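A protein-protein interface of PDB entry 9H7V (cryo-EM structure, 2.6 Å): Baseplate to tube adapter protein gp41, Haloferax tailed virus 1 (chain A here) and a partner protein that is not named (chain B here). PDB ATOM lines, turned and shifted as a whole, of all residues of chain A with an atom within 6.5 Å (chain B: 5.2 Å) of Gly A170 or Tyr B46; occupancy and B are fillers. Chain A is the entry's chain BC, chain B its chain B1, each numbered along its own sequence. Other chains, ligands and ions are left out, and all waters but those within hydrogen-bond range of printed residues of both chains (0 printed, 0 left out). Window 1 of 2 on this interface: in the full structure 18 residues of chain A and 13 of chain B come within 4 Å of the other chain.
O of Gly A117 lies close to O of Ser B50 (3.1 Å).
N of Gly A117 is in hydrogen-bond range of O of Thr B47 (2.8 Å).
The backbone carbonyl oxygen of Gly A117 sits close to the backbone carbonyl oxygen of Ile B48 (3.5 Å).
The side-chain carboxylate of Asp B54 sits at hydrogen-bond distance from the side-chain hydroxyl of Ser A168 (2.7 Å).
The backbone carbonyl oxygen of Tyr B46 sits at hydrogen-bond distance from the backbone NH of Gly A170, at 3.1 Å.
The side-chain carboxylate (OD2) of Asp B54 is in hydrogen-bond range of the backbone NH (N) of Ser A169.
Printed residues of chain B within 4 Å of Ala A116: Tyr B46 (3.4 Å) and Thr B47 (3.3 Å).
Gly A170 touches just these residues of chain B: Leu B45 and Tyr B46.
Tyr B46 touches just these residues of chain A: Ala A116, Gly A117, Ser A168, Gly A170 and Leu A171.
Of the printed residues of chain A, Thr B47 touches Ala A116, Gly A117, Ser A168 and Leu A171.
Of the printed residues of chain A, Asp B54 touches Ser A168 and Ser A169.
The nearest residue of chain B that does not touch Gly A170 is Thr B47 (5.0 Å).
The nearest residue of chain A that does not touch Tyr B46 is Ser A169 (4.2 Å).
Among the printed residues, pairs that only touch across the chains: Leu A171 with Ile B48 (3.1 Å), Ser A168 with Thr B47 (3.3 Å), Ala A116 with Thr B47 (3.3 Å), Gly A117 with Tyr B46 (3.4 Å), Ala A116 with Tyr B46 (3.4 Å), Leu A171 with Tyr B46 (3.5 Å), Glu A211 with Leu B45 (3.7 Å), Ser A168 with Tyr B46 (3.8 Å), Ser A172 with Ile B48 (3.8 Å), Leu A213 with Leu B45 (3.8 Å), Leu A171 with Thr B47 (3.9 Å) and Gly A170 with Leu B45 (3.9 Å).
Of the 13 printed residues of chain A, 9 touch a printed residue of chain B.
Hydrophobic or aromatic side chains of chain A that line the printed part of chain B: Ala A116 and Leu A213.
Of the 10 printed residues of chain B, 6 touch a printed residue of chain A.
The side-chain hydroxyl of Ser B50 is in hydrogen-bond range of the backbone NH of Phe B52, 3.0 Å away.
The side-chain hydroxyl (OG) of Ser A169 is in hydrogen-bond range of the backbone carbonyl oxygen (O) of Glu A211 (2.6 Å).
The backbone carbonyl oxygen (O) of Leu B45 lies within hydrogen-bond range of the backbone NH (N) of Asp B54 (2.7 Å).
The backbone carbonyl oxygen (O) of Ser A209 lies within hydrogen-bond range of the backbone NH (N) of Ser A172, 2.8 Å away.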
ATOM      1  N   ALA A 116       8.845   1.133 -13.552  1.00  0.00           N
ATOM      2  CA  ALA A 116       8.749  -0.260 -13.144  1.00  0.00           C
ATOM      3  C   ALA A 116       9.727  -0.528 -12.002  1.00  0.00           C
ATOM      4  O   ALA A 116      10.836   0.005 -11.991  1.00  0.00           O
ATOM      5  CB  ALA A 116       9.011  -1.161 -14.324  1.00  0.00           C
ATOM      6  N   GLY A 117       9.303  -1.377 -11.057  1.00  0.00           N
ATOM      7  CA  GLY A 117       9.911  -1.449  -9.738  1.00  0.00           C
ATOM      8  C   GLY A 117       9.387  -0.305  -8.875  1.00  0.00           C
ATOM      9  O   GLY A 117       8.190  -0.025  -8.893  1.00  0.00           O
ATOM     10  N   ARG A 118      10.291   0.319  -8.109  1.00  0.00           N
ATOM     11  CA  ARG A 118      10.179   1.699  -7.652  1.00  0.00           C
ATOM     12  C   ARG A 118       8.817   2.006  -7.025  1.00  0.00           C
ATOM     13  O   ARG A 118       8.185   2.996  -7.391  1.00  0.00           O
ATOM     14  CB  ARG A 118      10.457   2.656  -8.818  1.00  0.00           C
ATOM     15  CG  ARG A 118      11.894   2.657  -9.320  1.00  0.00           C
ATOM     16  CD  ARG A 118      12.752   3.661  -8.577  1.00  0.00           C
ATOM     17  NE  ARG A 118      14.059   3.805  -9.203  1.00  0.00           N
ATOM     18  CZ  ARG A 118      14.482   4.877  -9.867  1.00  0.00           C
ATOM     19  NH1 ARG A 118      15.695   4.881 -10.392  1.00  0.00           N
ATOM     20  NH2 ARG A 118      13.708   5.940 -10.000  1.00  0.00           N
ATOM     21  N   PRO A 167      -0.751  -5.229 -20.319  1.00  0.00           N
ATOM     22  CA  PRO A 167       0.152  -6.092 -19.552  1.00  0.00           C
ATOM     23  C   PRO A 167       0.846  -5.369 -18.400  1.00  0.00           C
ATOM     24  O   PRO A 167       1.325  -4.246 -18.561  1.00  0.00           O
ATOM     25  CB  PRO A 167       1.194  -6.535 -20.590  1.00  0.00           C
ATOM     26  CG  PRO A 167       0.457  -6.460 -21.907  1.00  0.00           C
ATOM     27  CD  PRO A 167      -0.459  -5.265 -21.762  1.00  0.00           C
ATOM     28  N   SER A 168       0.878  -6.039 -17.241  1.00  0.00           N
ATOM     29  CA  SER A 168       1.540  -5.562 -16.037  1.00  0.00           C
ATOM     30  C   SER A 168       3.058  -5.646 -16.187  1.00  0.00           C
ATOM     31  O   SER A 168       3.791  -4.933 -15.504  1.00  0.00           O
ATOM     32  CB  SER A 168       1.066  -6.334 -14.831  1.00  0.00           C
ATOM     33  OG  SER A 168       1.203  -7.733 -15.039  1.00  0.00           O
ATOM     34  N   SER A 169       3.504  -6.520 -17.098  1.00  0.00           N
ATOM     35  CA  SER A 169       4.901  -6.864 -17.314  1.00  0.00           C
ATOM     36  C   SER A 169       5.666  -5.700 -17.937  1.00  0.00           C
ATOM     37  O   SER A 169       5.407  -5.315 -19.076  1.00  0.00           O
ATOM     38  CB  SER A 169       5.010  -8.109 -18.152  1.00  0.00           C
ATOM     39  OG  SER A 169       4.144  -8.043 -19.274  1.00  0.00           O
ATOM     40  N   GLY A 170       6.608  -5.152 -17.159  1.00  0.00           N
ATOM     41  CA  GLY A 170       7.448  -4.041 -17.575  1.00  0.00           C
ATOM     42  C   GLY A 170       6.692  -2.716 -17.637  1.00  0.00           C
ATOM     43  O   GLY A 170       7.191  -1.764 -18.236  1.00  0.00           O
ATOM     44  N   LEU A 171       5.504  -2.662 -17.014  1.00  0.00           N
ATOM     45  CA  LEU A 171       4.625  -1.506 -17.110  1.00  0.00           C
ATOM     46  C   LEU A 171       5.271  -0.298 -16.435  1.00  0.00           C
ATOM     47  O   LEU A 171       5.696  -0.373 -15.285  1.00  0.00           O
ATOM     48  CB  LEU A 171       3.245  -1.827 -16.522  1.00  0.00           C
ATOM     49  CG  LEU A 171       2.174  -0.745 -16.684  1.00  0.00           C
ATOM     50  CD1 LEU A 171       1.778  -0.560 -18.143  1.00  0.00           C
ATOM     51  CD2 LEU A 171       0.949  -1.066 -15.843  1.00  0.00           C
ATOM     52  N   SER A 172       5.374   0.787 -17.210  1.00  0.00           N
ATOM     53  CA  SER A 172       5.787   2.100 -16.745  1.00  0.00           C
ATOM     54  C   SER A 172       4.726   3.115 -17.155  1.00  0.00           C
ATOM     55  O   SER A 172       4.146   3.001 -18.235  1.00  0.00           O
ATOM     56  CB  SER A 172       7.129   2.479 -17.313  1.00  0.00           C
ATOM     57  OG  SER A 172       8.111   1.504 -16.998  1.00  0.00           O
ATOM     58  N   SER A 209       4.574   2.345 -21.243  1.00  0.00           N
ATOM     59  CA  SER A 209       5.580   1.446 -21.779  1.00  0.00           C
ATOM     60  C   SER A 209       5.366   0.079 -21.139  1.00  0.00           C
ATOM     61  O   SER A 209       5.213  -0.003 -19.922  1.00  0.00           O
ATOM     62  CB  SER A 209       6.959   1.979 -21.486  1.00  0.00           C
ATOM     63  OG  SER A 209       7.944   1.293 -22.243  1.00  0.00           O
ATOM     64  N   PHE A 210       5.332  -0.981 -21.959  1.00  0.00           N
ATOM     65  CA  PHE A 210       5.090  -2.325 -21.454  1.00  0.00           C
ATOM     66  C   PHE A 210       5.607  -3.383 -22.423  1.00  0.00           C
ATOM     67  O   PHE A 210       5.944  -3.082 -23.567  1.00  0.00           O
ATOM     68  CB  PHE A 210       3.609  -2.543 -21.123  1.00  0.00           C
ATOM     69  CG  PHE A 210       2.632  -2.341 -22.254  1.00  0.00           C
ATOM     70  CD1 PHE A 210       2.304  -3.382 -23.113  1.00  0.00           C
ATOM     71  CD2 PHE A 210       2.009  -1.113 -22.440  1.00  0.00           C
ATOM     72  CE1 PHE A 210       1.391  -3.195 -24.142  1.00  0.00           C
ATOM     73  CE2 PHE A 210       1.100  -0.925 -23.471  1.00  0.00           C
ATOM     74  CZ  PHE A 210       0.793  -1.966 -24.320  1.00  0.00           C
ATOM     75  N   GLU A 211       5.653  -4.629 -21.933  1.00  0.00           N
ATOM     76  CA  GLU A 211       6.062  -5.775 -22.728  1.00  0.00           C
ATOM     77  C   GLU A 211       4.926  -6.798 -22.739  1.00  0.00           C
ATOM     78  O   GLU A 211       4.473  -7.241 -21.686  1.00  0.00           O
ATOM     79  CB  GLU A 211       7.428  -6.290 -22.261  1.00  0.00           C
ATOM     80  CG  GLU A 211       8.475  -5.182 -22.205  1.00  0.00           C
ATOM     81  CD  GLU A 211       9.953  -5.533 -22.253  1.00  0.00           C
ATOM     82  OE1 GLU A 211      10.295  -6.626 -22.733  1.00  0.00           O
ATOM     83  OE2 GLU A 211      10.765  -4.695 -21.810  1.00  0.00           O
ATOM     84  N   LEU A 213       3.542 -10.272 -23.225  1.00  0.00           N
ATOM     85  CA  LEU A 213       4.216 -11.545 -23.020  1.00  0.00           C
ATOM     86  C   LEU A 213       3.363 -12.722 -23.486  1.00  0.00           C
ATOM     87  O   LEU A 213       3.900 -13.672 -24.053  1.00  0.00           O
ATOM     88  CB  LEU A 213       4.622 -11.694 -21.550  1.00  0.00           C
ATOM     89  CG  LEU A 213       5.670 -10.714 -21.019  1.00  0.00           C
ATOM     90  CD1 LEU A 213       6.089 -11.114 -19.617  1.00  0.00           C
ATOM     91  CD2 LEU A 213       6.892 -10.644 -21.925  1.00  0.00           C
ATOM     92  N   GLU B  44      14.161  -9.801 -16.777  1.00  0.00           N
ATOM     93  CA  GLU B  44      13.419  -9.720 -15.529  1.00  0.00           C
ATOM     94  C   GLU B  44      12.588  -8.440 -15.528  1.00  0.00           C
ATOM     95  O   GLU B  44      13.132  -7.344 -15.672  1.00  0.00           O
ATOM     96  CB  GLU B  44      14.369  -9.776 -14.330  1.00  0.00           C
ATOM     97  CG  GLU B  44      15.004 -11.138 -14.117  1.00  0.00           C
ATOM     98  CD  GLU B  44      15.803 -11.267 -12.832  1.00  0.00           C
ATOM     99  OE1 GLU B  44      16.858 -10.611 -12.720  1.00  0.00           O
ATOM    100  OE2 GLU B  44      15.361 -12.015 -11.941  1.00  0.00           O
ATOM    101  N   LEU B  45      11.270  -8.599 -15.359  1.00  0.00           N
ATOM    102  CA  LEU B  45      10.311  -7.526 -15.582  1.00  0.00           C
ATOM    103  C   LEU B  45       9.554  -7.210 -14.292  1.00  0.00           C
ATOM    104  O   LEU B  45       9.224  -8.113 -13.527  1.00  0.00           O
ATOM    105  CB  LEU B  45       9.366  -7.935 -16.719  1.00  0.00           C
ATOM    106  CG  LEU B  45      10.012  -8.102 -18.097  1.00  0.00           C
ATOM    107  CD1 LEU B  45       9.180  -9.012 -18.985  1.00  0.00           C
ATOM    108  CD2 LEU B  45      10.238  -6.757 -18.773  1.00  0.00           C
ATOM    109  N   TYR B  46       9.279  -5.913 -14.080  1.00  0.00           N
ATOM    110  CA  TYR B  46       8.690  -5.380 -12.857  1.00  0.00           C
ATOM    111  C   TYR B  46       7.442  -4.557 -13.206  1.00  0.00           C
ATOM    112  O   TYR B  46       7.297  -4.133 -14.350  1.00  0.00           O
ATOM    113  CB  TYR B  46       9.755  -4.579 -12.094  1.00  0.00           C
ATOM    114  CG  TYR B  46      10.916  -5.379 -11.548  1.00  0.00           C
ATOM    115  CD1 TYR B  46      12.009  -5.718 -12.339  1.00  0.00           C
ATOM    116  CD2 TYR B  46      10.936  -5.786 -10.222  1.00  0.00           C
ATOM    117  CE1 TYR B  46      13.072  -6.454 -11.833  1.00  0.00           C
ATOM    118  CE2 TYR B  46      11.992  -6.519  -9.699  1.00  0.00           C
ATOM    119  CZ  TYR B  46      13.065  -6.856 -10.508  1.00  0.00           C
ATOM    120  OH  TYR B  46      14.109  -7.575 -10.000  1.00  0.00           O
ATOM    121  N   THR B  47       6.539  -4.342 -12.230  1.00  0.00           N
ATOM    122  CA  THR B  47       5.330  -3.536 -12.417  1.00  0.00           C
ATOM    123  C   THR B  47       5.508  -2.153 -11.783  1.00  0.00           C
ATOM    124  O   THR B  47       6.557  -1.874 -11.203  1.00  0.00           O
ATOM    125  CB  THR B  47       4.059  -4.216 -11.877  1.00  0.00           C
ATOM    126  OG1 THR B  47       4.003  -4.093 -10.455  1.00  0.00           O
ATOM    127  CG2 THR B  47       3.913  -5.668 -12.272  1.00  0.00           C
ATOM    128  N   ILE B  48       4.461  -1.311 -11.861  1.00  0.00           N
ATOM    129  CA  ILE B  48       4.517   0.092 -11.458  1.00  0.00           C
ATOM    130  C   ILE B  48       4.488   0.270  -9.938  1.00  0.00           C
ATOM    131  O   ILE B  48       5.023   1.259  -9.436  1.00  0.00           O
ATOM    132  CB  ILE B  48       3.451   0.973 -12.154  1.00  0.00           C
ATOM    133  CG1 ILE B  48       2.066   0.316 -12.207  1.00  0.00           C
ATOM    134  CG2 ILE B  48       3.928   1.432 -13.522  1.00  0.00           C
ATOM    135  CD1 ILE B  48       0.927   1.267 -12.525  1.00  0.00           C
ATOM    136  N   SER B  50       5.265  -2.084  -7.320  1.00  0.00           N
ATOM    137  CA  SER B  50       5.867  -3.194  -6.598  1.00  0.00           C
ATOM    138  C   SER B  50       7.376  -3.222  -6.818  1.00  0.00           C
ATOM    139  O   SER B  50       7.848  -2.941  -7.917  1.00  0.00           O
ATOM    140  CB  SER B  50       5.233  -4.500  -7.010  1.00  0.00           C
ATOM    141  OG  SER B  50       5.861  -5.601  -6.370  1.00  0.00           O
ATOM    142  N   THR B  51       8.108  -3.593  -5.760  1.00  0.00           N
ATOM    143  CA  THR B  51       9.544  -3.822  -5.805  1.00  0.00           C
ATOM    144  C   THR B  51       9.835  -5.228  -6.333  1.00  0.00           C
ATOM    145  O   THR B  51      10.965  -5.520  -6.721  1.00  0.00           O
ATOM    146  CB  THR B  51      10.193  -3.627  -4.428  1.00  0.00           C
ATOM    147  OG1 THR B  51       9.589  -4.511  -3.484  1.00  0.00           O
ATOM    148  CG2 THR B  51      10.127  -2.200  -3.927  1.00  0.00           C
ATOM    149  N   PHE B  52       8.803  -6.083  -6.346  1.00  0.00           N
ATOM    150  CA  PHE B  52       8.935  -7.491  -6.687  1.00  0.00           C
ATOM    151  C   PHE B  52       8.782  -7.694  -8.194  1.00  0.00           C
ATOM    152  O   PHE B  52       8.123  -6.910  -8.874  1.00  0.00           O
ATOM    153  CB  PHE B  52       7.897  -8.321  -5.925  1.00  0.00           C
ATOM    154  CG  PHE B  52       8.125  -8.552  -4.449  1.00  0.00           C
ATOM    155  CD1 PHE B  52       9.157  -7.936  -3.748  1.00  0.00           C
ATOM    156  CD2 PHE B  52       7.262  -9.378  -3.743  1.00  0.00           C
ATOM    157  CE1 PHE B  52       9.329  -8.160  -2.389  1.00  0.00           C
ATOM    158  CE2 PHE B  52       7.431  -9.601  -2.383  1.00  0.00           C
ATOM    159  CZ  PHE B  52       8.466  -8.992  -1.708  1.00  0.00           C
ATOM    160  N   ARG B  53       9.396  -8.780  -8.682  1.00  0.00           N
ATOM    161  CA  ARG B  53       9.456  -9.165 -10.083  1.00  0.00           C
ATOM    162  C   ARG B  53       8.100  -9.723 -10.514  1.00  0.00           C
ATOM    163  O   ARG B  53       7.542 -10.587  -9.841  1.00  0.00           O
ATOM    164  CB  ARG B  53      10.572 -10.205 -10.234  1.00  0.00           C
ATOM    165  CG  ARG B  53      11.004 -10.511 -11.660  1.00  0.00           C
ATOM    166  CD  ARG B  53      12.086 -11.577 -11.667  1.00  0.00           C
ATOM    167  NE  ARG B  53      11.589 -12.875 -11.223  1.00  0.00           N
ATOM    168  CZ  ARG B  53      12.334 -13.908 -10.835  1.00  0.00           C
ATOM    169  NH1 ARG B  53      11.745 -15.029 -10.457  1.00  0.00           N
ATOM    170  NH2 ARG B  53      13.653 -13.826 -10.821  1.00  0.00           N
ATOM    171  N   ASP B  54       7.587  -9.213 -11.642  1.00  0.00           N
ATOM    172  CA  ASP B  54       6.322  -9.658 -12.207  1.00  0.00           C
ATOM    173  C   ASP B  54       6.537 -10.959 -12.972  1.00  0.00           C
ATOM    174  O   ASP B  54       5.874 -11.959 -12.699  1.00  0.00           O
ATOM    175  CB  ASP B  54       5.691  -8.588 -13.102  1.00  0.00           C
ATOM    176  CG  ASP B  54       4.229  -8.843 -13.443  1.00  0.00           C
ATOM    177  OD1 ASP B  54       3.527  -9.473 -12.623  1.00  0.00           O
ATOM    178  OD2 ASP B  54       3.796  -8.395 -14.522  1.00  0.00           O
